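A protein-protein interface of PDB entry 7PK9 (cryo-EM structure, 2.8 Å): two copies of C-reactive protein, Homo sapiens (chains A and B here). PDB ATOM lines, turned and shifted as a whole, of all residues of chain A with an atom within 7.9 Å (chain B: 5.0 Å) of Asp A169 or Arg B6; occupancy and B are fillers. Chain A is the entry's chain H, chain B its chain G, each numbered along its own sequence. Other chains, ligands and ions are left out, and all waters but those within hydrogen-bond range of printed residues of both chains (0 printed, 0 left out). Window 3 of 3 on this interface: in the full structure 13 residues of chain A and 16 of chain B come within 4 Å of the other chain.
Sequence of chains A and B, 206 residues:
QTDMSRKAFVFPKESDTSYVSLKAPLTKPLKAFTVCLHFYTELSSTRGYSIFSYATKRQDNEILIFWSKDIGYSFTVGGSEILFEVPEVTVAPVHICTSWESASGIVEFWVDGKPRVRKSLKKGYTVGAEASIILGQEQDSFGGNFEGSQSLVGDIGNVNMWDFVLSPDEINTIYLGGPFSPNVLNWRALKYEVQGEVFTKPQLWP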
ATOM      1  N   TRP A 110     -21.516  -1.221  -8.953  1.00  0.00           N
ATOM      2  CA  TRP A 110     -21.382  -1.090 -10.398  1.00  0.00           C
ATOM      3  C   TRP A 110     -20.900   0.313 -10.698  1.00  0.00           C
ATOM      4  O   TRP A 110     -21.496   1.285 -10.238  1.00  0.00           O
ATOM      5  CB  TRP A 110     -22.726  -1.311 -11.088  1.00  0.00           C
ATOM      6  CG  TRP A 110     -23.239  -2.675 -11.022  1.00  0.00           C
ATOM      7  CD1 TRP A 110     -23.820  -3.280  -9.963  1.00  0.00           C
ATOM      8  CD2 TRP A 110     -23.235  -3.625 -12.081  1.00  0.00           C
ATOM      9  NE1 TRP A 110     -24.171  -4.561 -10.290  1.00  0.00           N
ATOM     10  CE2 TRP A 110     -23.835  -4.789 -11.594  1.00  0.00           C
ATOM     11  CE3 TRP A 110     -22.778  -3.602 -13.397  1.00  0.00           C
ATOM     12  CZ2 TRP A 110     -23.993  -5.917 -12.372  1.00  0.00           C
ATOM     13  CZ3 TRP A 110     -22.941  -4.717 -14.165  1.00  0.00           C
ATOM     14  CH2 TRP A 110     -23.538  -5.861 -13.654  1.00  0.00           C
ATOM     15  N   ARG A 118     -18.591  -8.821  -5.996  1.00  0.00           N
ATOM     16  CA  ARG A 118     -19.514  -8.831  -4.863  1.00  0.00           C
ATOM     17  C   ARG A 118     -18.819  -9.055  -3.523  1.00  0.00           C
ATOM     18  O   ARG A 118     -17.975  -9.941  -3.379  1.00  0.00           O
ATOM     19  CB  ARG A 118     -20.591  -9.887  -5.092  1.00  0.00           C
ATOM     20  CG  ARG A 118     -21.687  -9.370  -5.986  1.00  0.00           C
ATOM     21  CD  ARG A 118     -22.841 -10.328  -6.177  1.00  0.00           C
ATOM     22  NE  ARG A 118     -22.655 -11.263  -7.277  1.00  0.00           N
ATOM     23  CZ  ARG A 118     -23.576 -11.549  -8.194  1.00  0.00           C
ATOM     24  NH1 ARG A 118     -24.693 -10.848  -8.289  1.00  0.00           N
ATOM     25  NH2 ARG A 118     -23.293 -12.425  -9.142  1.00  0.00           N
ATOM     26  N   LEU A 166     -31.587  -4.630  -7.864  1.00  0.00           N
ATOM     27  CA  LEU A 166     -31.682  -4.782  -9.307  1.00  0.00           C
ATOM     28  C   LEU A 166     -30.765  -5.893  -9.794  1.00  0.00           C
ATOM     29  O   LEU A 166     -29.643  -6.049  -9.310  1.00  0.00           O
ATOM     30  CB  LEU A 166     -31.318  -3.474  -9.999  1.00  0.00           C
ATOM     31  CG  LEU A 166     -32.252  -2.292  -9.767  1.00  0.00           C
ATOM     32  CD1 LEU A 166     -31.862  -1.164 -10.688  1.00  0.00           C
ATOM     33  CD2 LEU A 166     -33.696  -2.673  -9.967  1.00  0.00           C
ATOM     34  N   SER A 167     -31.242  -6.661 -10.768  1.00  0.00           N
ATOM     35  CA  SER A 167     -30.408  -7.634 -11.446  1.00  0.00           C
ATOM     36  C   SER A 167     -29.377  -6.947 -12.343  1.00  0.00           C
ATOM     37  O   SER A 167     -29.478  -5.757 -12.634  1.00  0.00           O
ATOM     38  CB  SER A 167     -31.279  -8.592 -12.251  1.00  0.00           C
ATOM     39  OG  SER A 167     -31.986  -7.911 -13.263  1.00  0.00           O
ATOM     40  N   PRO A 168     -28.363  -7.685 -12.786  1.00  0.00           N
ATOM     41  CA  PRO A 168     -27.431  -7.159 -13.798  1.00  0.00           C
ATOM     42  C   PRO A 168     -28.068  -6.642 -15.081  1.00  0.00           C
ATOM     43  O   PRO A 168     -27.627  -5.613 -15.600  1.00  0.00           O
ATOM     44  CB  PRO A 168     -26.518  -8.361 -14.060  1.00  0.00           C
ATOM     45  CG  PRO A 168     -26.514  -9.082 -12.776  1.00  0.00           C
ATOM     46  CD  PRO A 168     -27.921  -8.993 -12.288  1.00  0.00           C
ATOM     47  N   ASP A 169     -29.072  -7.330 -15.621  1.00  0.00           N
ATOM     48  CA  ASP A 169     -29.780  -6.823 -16.795  1.00  0.00           C
ATOM     49  C   ASP A 169     -30.441  -5.487 -16.512  1.00  0.00           C
ATOM     50  O   ASP A 169     -30.327  -4.544 -17.298  1.00  0.00           O
ATOM     51  CB  ASP A 169     -30.844  -7.819 -17.240  1.00  0.00           C
ATOM     52  CG  ASP A 169     -30.265  -9.044 -17.874  1.00  0.00           C
ATOM     53  OD1 ASP A 169     -29.074  -9.019 -18.254  1.00  0.00           O
ATOM     54  OD2 ASP A 169     -31.006 -10.042 -17.998  1.00  0.00           O
ATOM     55  N   GLU A 170     -31.146  -5.394 -15.393  1.00  0.00           N
ATOM     56  CA  GLU A 170     -31.800  -4.152 -15.011  1.00  0.00           C
ATOM     57  C   GLU A 170     -30.806  -3.005 -14.887  1.00  0.00           C
ATOM     58  O   GLU A 170     -31.071  -1.895 -15.355  1.00  0.00           O
ATOM     59  CB  GLU A 170     -32.549  -4.386 -13.705  1.00  0.00           C
ATOM     60  CG  GLU A 170     -33.767  -5.279 -13.896  1.00  0.00           C
ATOM     61  CD  GLU A 170     -34.431  -5.689 -12.596  1.00  0.00           C
ATOM     62  OE1 GLU A 170     -33.888  -5.395 -11.515  1.00  0.00           O
ATOM     63  OE2 GLU A 170     -35.503  -6.315 -12.658  1.00  0.00           O
ATOM     64  N   ILE A 171     -29.654  -3.253 -14.271  1.00  0.00           N
ATOM     65  CA  ILE A 171     -28.621  -2.227 -14.156  1.00  0.00           C
ATOM     66  C   ILE A 171     -28.091  -1.798 -15.519  1.00  0.00           C
ATOM     67  O   ILE A 171     -27.830  -0.614 -15.746  1.00  0.00           O
ATOM     68  CB  ILE A 171     -27.488  -2.719 -13.240  1.00  0.00           C
ATOM     69  CG1 ILE A 171     -28.012  -2.820 -11.813  1.00  0.00           C
ATOM     70  CG2 ILE A 171     -26.290  -1.790 -13.335  1.00  0.00           C
ATOM     71  CD1 ILE A 171     -27.042  -3.382 -10.840  1.00  0.00           C
ATOM     72  N   ASN A 172     -27.897  -2.740 -16.436  1.00  0.00           N
ATOM     73  CA  ASN A 172     -27.511  -2.379 -17.798  1.00  0.00           C
ATOM     74  C   ASN A 172     -28.525  -1.463 -18.472  1.00  0.00           C
ATOM     75  O   ASN A 172     -28.143  -0.536 -19.190  1.00  0.00           O
ATOM     76  CB  ASN A 172     -27.313  -3.636 -18.640  1.00  0.00           C
ATOM     77  CG  ASN A 172     -26.175  -4.501 -18.152  1.00  0.00           C
ATOM     78  OD1 ASN A 172     -26.203  -5.718 -18.317  1.00  0.00           O
ATOM     79  ND2 ASN A 172     -25.151  -3.885 -17.584  1.00  0.00           N
ATOM     80  N   THR A 173     -29.818  -1.714 -18.283  1.00  0.00           N
ATOM     81  CA  THR A 173     -30.810  -0.783 -18.810  1.00  0.00           C
ATOM     82  C   THR A 173     -30.748   0.585 -18.136  1.00  0.00           C
ATOM     83  O   THR A 173     -30.999   1.596 -18.795  1.00  0.00           O
ATOM     84  CB  THR A 173     -32.214  -1.367 -18.684  1.00  0.00           C
ATOM     85  OG1 THR A 173     -32.567  -1.494 -17.304  1.00  0.00           O
ATOM     86  CG2 THR A 173     -32.289  -2.725 -19.352  1.00  0.00           C
ATOM     87  N   ILE A 174     -30.410   0.660 -16.849  1.00  0.00           N
ATOM     88  CA  ILE A 174     -30.206   1.973 -16.239  1.00  0.00           C
ATOM     89  C   ILE A 174     -29.071   2.702 -16.942  1.00  0.00           C
ATOM     90  O   ILE A 174     -29.220   3.845 -17.386  1.00  0.00           O
ATOM     91  CB  ILE A 174     -29.921   1.849 -14.731  1.00  0.00           C
ATOM     92  CG1 ILE A 174     -30.899   0.921 -14.014  1.00  0.00           C
ATOM     93  CG2 ILE A 174     -29.982   3.204 -14.075  1.00  0.00           C
ATOM     94  CD1 ILE A 174     -32.324   1.178 -14.287  1.00  0.00           C
ATOM     95  N   TYR A 175     -27.918   2.047 -17.059  1.00  0.00           N
ATOM     96  CA  TYR A 175     -26.736   2.717 -17.587  1.00  0.00           C
ATOM     97  C   TYR A 175     -26.912   3.113 -19.043  1.00  0.00           C
ATOM     98  O   TYR A 175     -26.550   4.227 -19.434  1.00  0.00           O
ATOM     99  CB  TYR A 175     -25.523   1.813 -17.419  1.00  0.00           C
ATOM    100  CG  TYR A 175     -24.251   2.387 -17.965  1.00  0.00           C
ATOM    101  CD1 TYR A 175     -23.567   1.755 -18.983  1.00  0.00           C
ATOM    102  CD2 TYR A 175     -23.744   3.567 -17.469  1.00  0.00           C
ATOM    103  CE1 TYR A 175     -22.404   2.275 -19.477  1.00  0.00           C
ATOM    104  CE2 TYR A 175     -22.583   4.098 -17.957  1.00  0.00           C
ATOM    105  CZ  TYR A 175     -21.916   3.452 -18.962  1.00  0.00           C
ATOM    106  OH  TYR A 175     -20.760   3.993 -19.459  1.00  0.00           O
ATOM    107  N   LEU A 176     -27.469   2.228 -19.859  1.00  0.00           N
ATOM    108  CA  LEU A 176     -27.785   2.555 -21.241  1.00  0.00           C
ATOM    109  C   LEU A 176     -29.037   3.410 -21.373  1.00  0.00           C
ATOM    110  O   LEU A 176     -29.453   3.696 -22.496  1.00  0.00           O
ATOM    111  CB  LEU A 176     -27.934   1.277 -22.062  1.00  0.00           C
ATOM    112  CG  LEU A 176     -26.684   0.394 -22.059  1.00  0.00           C
ATOM    113  CD1 LEU A 176     -26.942  -0.920 -22.755  1.00  0.00           C
ATOM    114  CD2 LEU A 176     -25.509   1.106 -22.689  1.00  0.00           C
ATOM    115  N   MET B   4     -28.263 -24.159 -14.127  1.00  0.00           N
ATOM    116  CA  MET B   4     -27.634 -22.990 -13.535  1.00  0.00           C
ATOM    117  C   MET B   4     -27.366 -21.869 -14.532  1.00  0.00           C
ATOM    118  O   MET B   4     -26.654 -20.926 -14.191  1.00  0.00           O
ATOM    119  CB  MET B   4     -26.330 -23.414 -12.862  1.00  0.00           C
ATOM    120  CG  MET B   4     -26.534 -24.370 -11.700  1.00  0.00           C
ATOM    121  SD  MET B   4     -27.146 -23.636 -10.170  1.00  0.00           S
ATOM    122  CE  MET B   4     -26.245 -22.098 -10.076  1.00  0.00           C
ATOM    123  N   SER B   5     -27.917 -21.939 -15.739  1.00  0.00           N
ATOM    124  CA  SER B   5     -27.705 -20.896 -16.737  1.00  0.00           C
ATOM    125  C   SER B   5     -27.987 -19.501 -16.200  1.00  0.00           C
ATOM    126  O   SER B   5     -28.986 -19.265 -15.520  1.00  0.00           O
ATOM    127  CB  SER B   5     -28.597 -21.145 -17.952  1.00  0.00           C
ATOM    128  OG  SER B   5     -28.304 -22.383 -18.559  1.00  0.00           O
ATOM    129  N   ARG B   6     -27.086 -18.574 -16.527  1.00  0.00           N
ATOM    130  CA  ARG B   6     -27.059 -17.193 -16.050  1.00  0.00           C
ATOM    131  C   ARG B   6     -26.934 -17.038 -14.541  1.00  0.00           C
ATOM    132  O   ARG B   6     -27.193 -15.954 -14.024  1.00  0.00           O
ATOM    133  CB  ARG B   6     -28.276 -16.416 -16.543  1.00  0.00           C
ATOM    134  CG  ARG B   6     -28.438 -16.445 -18.049  1.00  0.00           C
ATOM    135  CD  ARG B   6     -29.420 -15.397 -18.491  1.00  0.00           C
ATOM    136  NE  ARG B   6     -28.805 -14.075 -18.425  1.00  0.00           N
ATOM    137  CZ  ARG B   6     -29.450 -12.945 -18.153  1.00  0.00           C
ATOM    138  NH1 ARG B   6     -30.728 -12.955 -17.803  1.00  0.00           N
ATOM    139  NH2 ARG B   6     -28.767 -11.815 -18.099  1.00  0.00           N
ATOM    140  N   LYS B   7     -26.587 -18.083 -13.808  1.00  0.00           N
ATOM    141  CA  LYS B   7     -26.405 -17.984 -12.370  1.00  0.00           C
ATOM    142  C   LYS B   7     -24.952 -18.267 -12.021  1.00  0.00           C
ATOM    143  O   LYS B   7     -24.264 -19.016 -12.716  1.00  0.00           O
ATOM    144  CB  LYS B   7     -27.326 -18.932 -11.621  1.00  0.00           C
ATOM    145  CG  LYS B   7     -28.781 -18.612 -11.799  1.00  0.00           C
ATOM    146  CD  LYS B   7     -29.648 -19.711 -11.249  1.00  0.00           C
ATOM    147  CE  LYS B   7     -31.110 -19.363 -11.387  1.00  0.00           C
ATOM    148  NZ  LYS B   7     -31.559 -19.497 -12.792  1.00  0.00           N
ATOM    149  N   ALA B   8     -24.489 -17.644 -10.943  1.00  0.00           N
ATOM    150  CA  ALA B   8     -23.150 -17.865 -10.427  1.00  0.00           C
ATOM    151  C   ALA B   8     -23.214 -18.218  -8.953  1.00  0.00           C
ATOM    152  O   ALA B   8     -24.125 -17.806  -8.237  1.00  0.00           O
ATOM    153  CB  ALA B   8     -22.266 -16.627 -10.614  1.00  0.00           C
ATOM    154  N   LYS B 201     -26.513 -16.448  -7.508  1.00  0.00           N
ATOM    155  CA  LYS B 201     -26.895 -15.108  -7.919  1.00  0.00           C
ATOM    156  C   LYS B 201     -26.811 -15.009  -9.431  1.00  0.00           C
ATOM    157  O   LYS B 201     -26.166 -15.839 -10.076  1.00  0.00           O
ATOM    158  CB  LYS B 201     -25.976 -14.052  -7.294  1.00  0.00           C
ATOM    159  CG  LYS B 201     -26.126 -13.865  -5.810  1.00  0.00           C
ATOM    160  CD  LYS B 201     -27.505 -13.387  -5.436  1.00  0.00           C
ATOM    161  CE  LYS B 201     -27.594 -13.141  -3.958  1.00  0.00           C
ATOM    162  NZ  LYS B 201     -28.544 -12.058  -3.627  1.00  0.00           N
ATOM    163  N   PRO B 202     -27.463 -14.014 -10.028  1.00  0.00           N
ATOM    164  CA  PRO B 202     -27.242 -13.744 -11.449  1.00  0.00           C
ATOM    165  C   PRO B 202     -25.775 -13.471 -11.743  1.00  0.00           C
ATOM    166  O   PRO B 202     -25.114 -12.716 -11.032  1.00  0.00           O
ATOM    167  CB  PRO B 202     -28.105 -12.505 -11.706  1.00  0.00           C
ATOM    168  CG  PRO B 202     -29.128 -12.554 -10.674  1.00  0.00           C
ATOM    169  CD  PRO B 202     -28.447 -13.085  -9.462  1.00  0.00           C
ATOM    170  N   GLN B 203     -25.269 -14.081 -12.808  1.00  0.00           N
ATOM    171  CA  GLN B 203     -23.867 -13.912 -13.153  1.00  0.00           C
ATOM    172  C   GLN B 203     -23.583 -12.475 -13.569  1.00  0.00           C
ATOM    173  O   GLN B 203     -24.357 -11.861 -14.306  1.00  0.00           O
ATOM    174  CB  GLN B 203     -23.492 -14.874 -14.277  1.00  0.00           C
ATOM    175  CG  GLN B 203     -23.982 -14.436 -15.628  1.00  0.00           C
ATOM    176  CD  GLN B 203     -23.720 -15.453 -16.700  1.00  0.00           C
ATOM    177  OE1 GLN B 203     -23.691 -16.651 -16.441  1.00  0.00           O
ATOM    178  NE2 GLN B 203     -23.549 -14.984 -17.920  1.00  0.00           N
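The guanidinium group (NH2) of Arg B6 is in salt-bridge range of the side-chain carboxylate (OD1) of Asp A169, at 2.8 Å.
The guanidinium group of Arg A118 sits at hydrogen-bond distance from the backbone carbonyl oxygen of Pro B202 (2.6 Å).
No position is printed for both chains.
Of the 5 pairs that touch across the chains among the printed residues, none has its exchanged pair printed and touching as well.
Hydrophobic or aromatic side chains of chain A that line the printed part of chain B: Pro A168.
Of the printed residues of chain B, Arg A118 touches Lys B201 and Pro B202.
Of the printed residues of chain B, Pro A168 touches Pro B202 (3.6 Å) and Gln B203 (3.8 Å).
Of chain B, only Arg B6 (2.8 Å) comes within 4 Å of Asp A169.
Of the printed residues of chain A, Arg B6 touches Asp A169 (2.8 Å).
Of the printed residues of chain A, Lys B201 touches Arg A118 (3.6 Å).
The nearest residue of chain A that does not touch Arg B6 is Pro A168 (5.8 Å).
The nearest printed residue of chain A that does not touch Gln B203 is Arg A118 (4.3 Å).
Among the printed residues, merely in contact across the chains: Pro A168 with Pro B202 (3.6 Å), Arg A118 with Lys B201 (3.6 Å) and Pro A168 with Gln B203 (3.8 Å).
The backbone carbonyl oxygen (O) of Arg B6 is in hydrogen-bond range of the backbone NH (N) of Gln B203, at 2.9 Å.
The backbone NH of Ala B8 sits at hydrogen-bond distance from the backbone carbonyl oxygen of Lys B201, 2.6 Å away.
The side-chain amide oxygen (OD1) of Asn A172 sits close to the backbone carbonyl oxygen (O) of Pro A168, 3.1 Å away.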
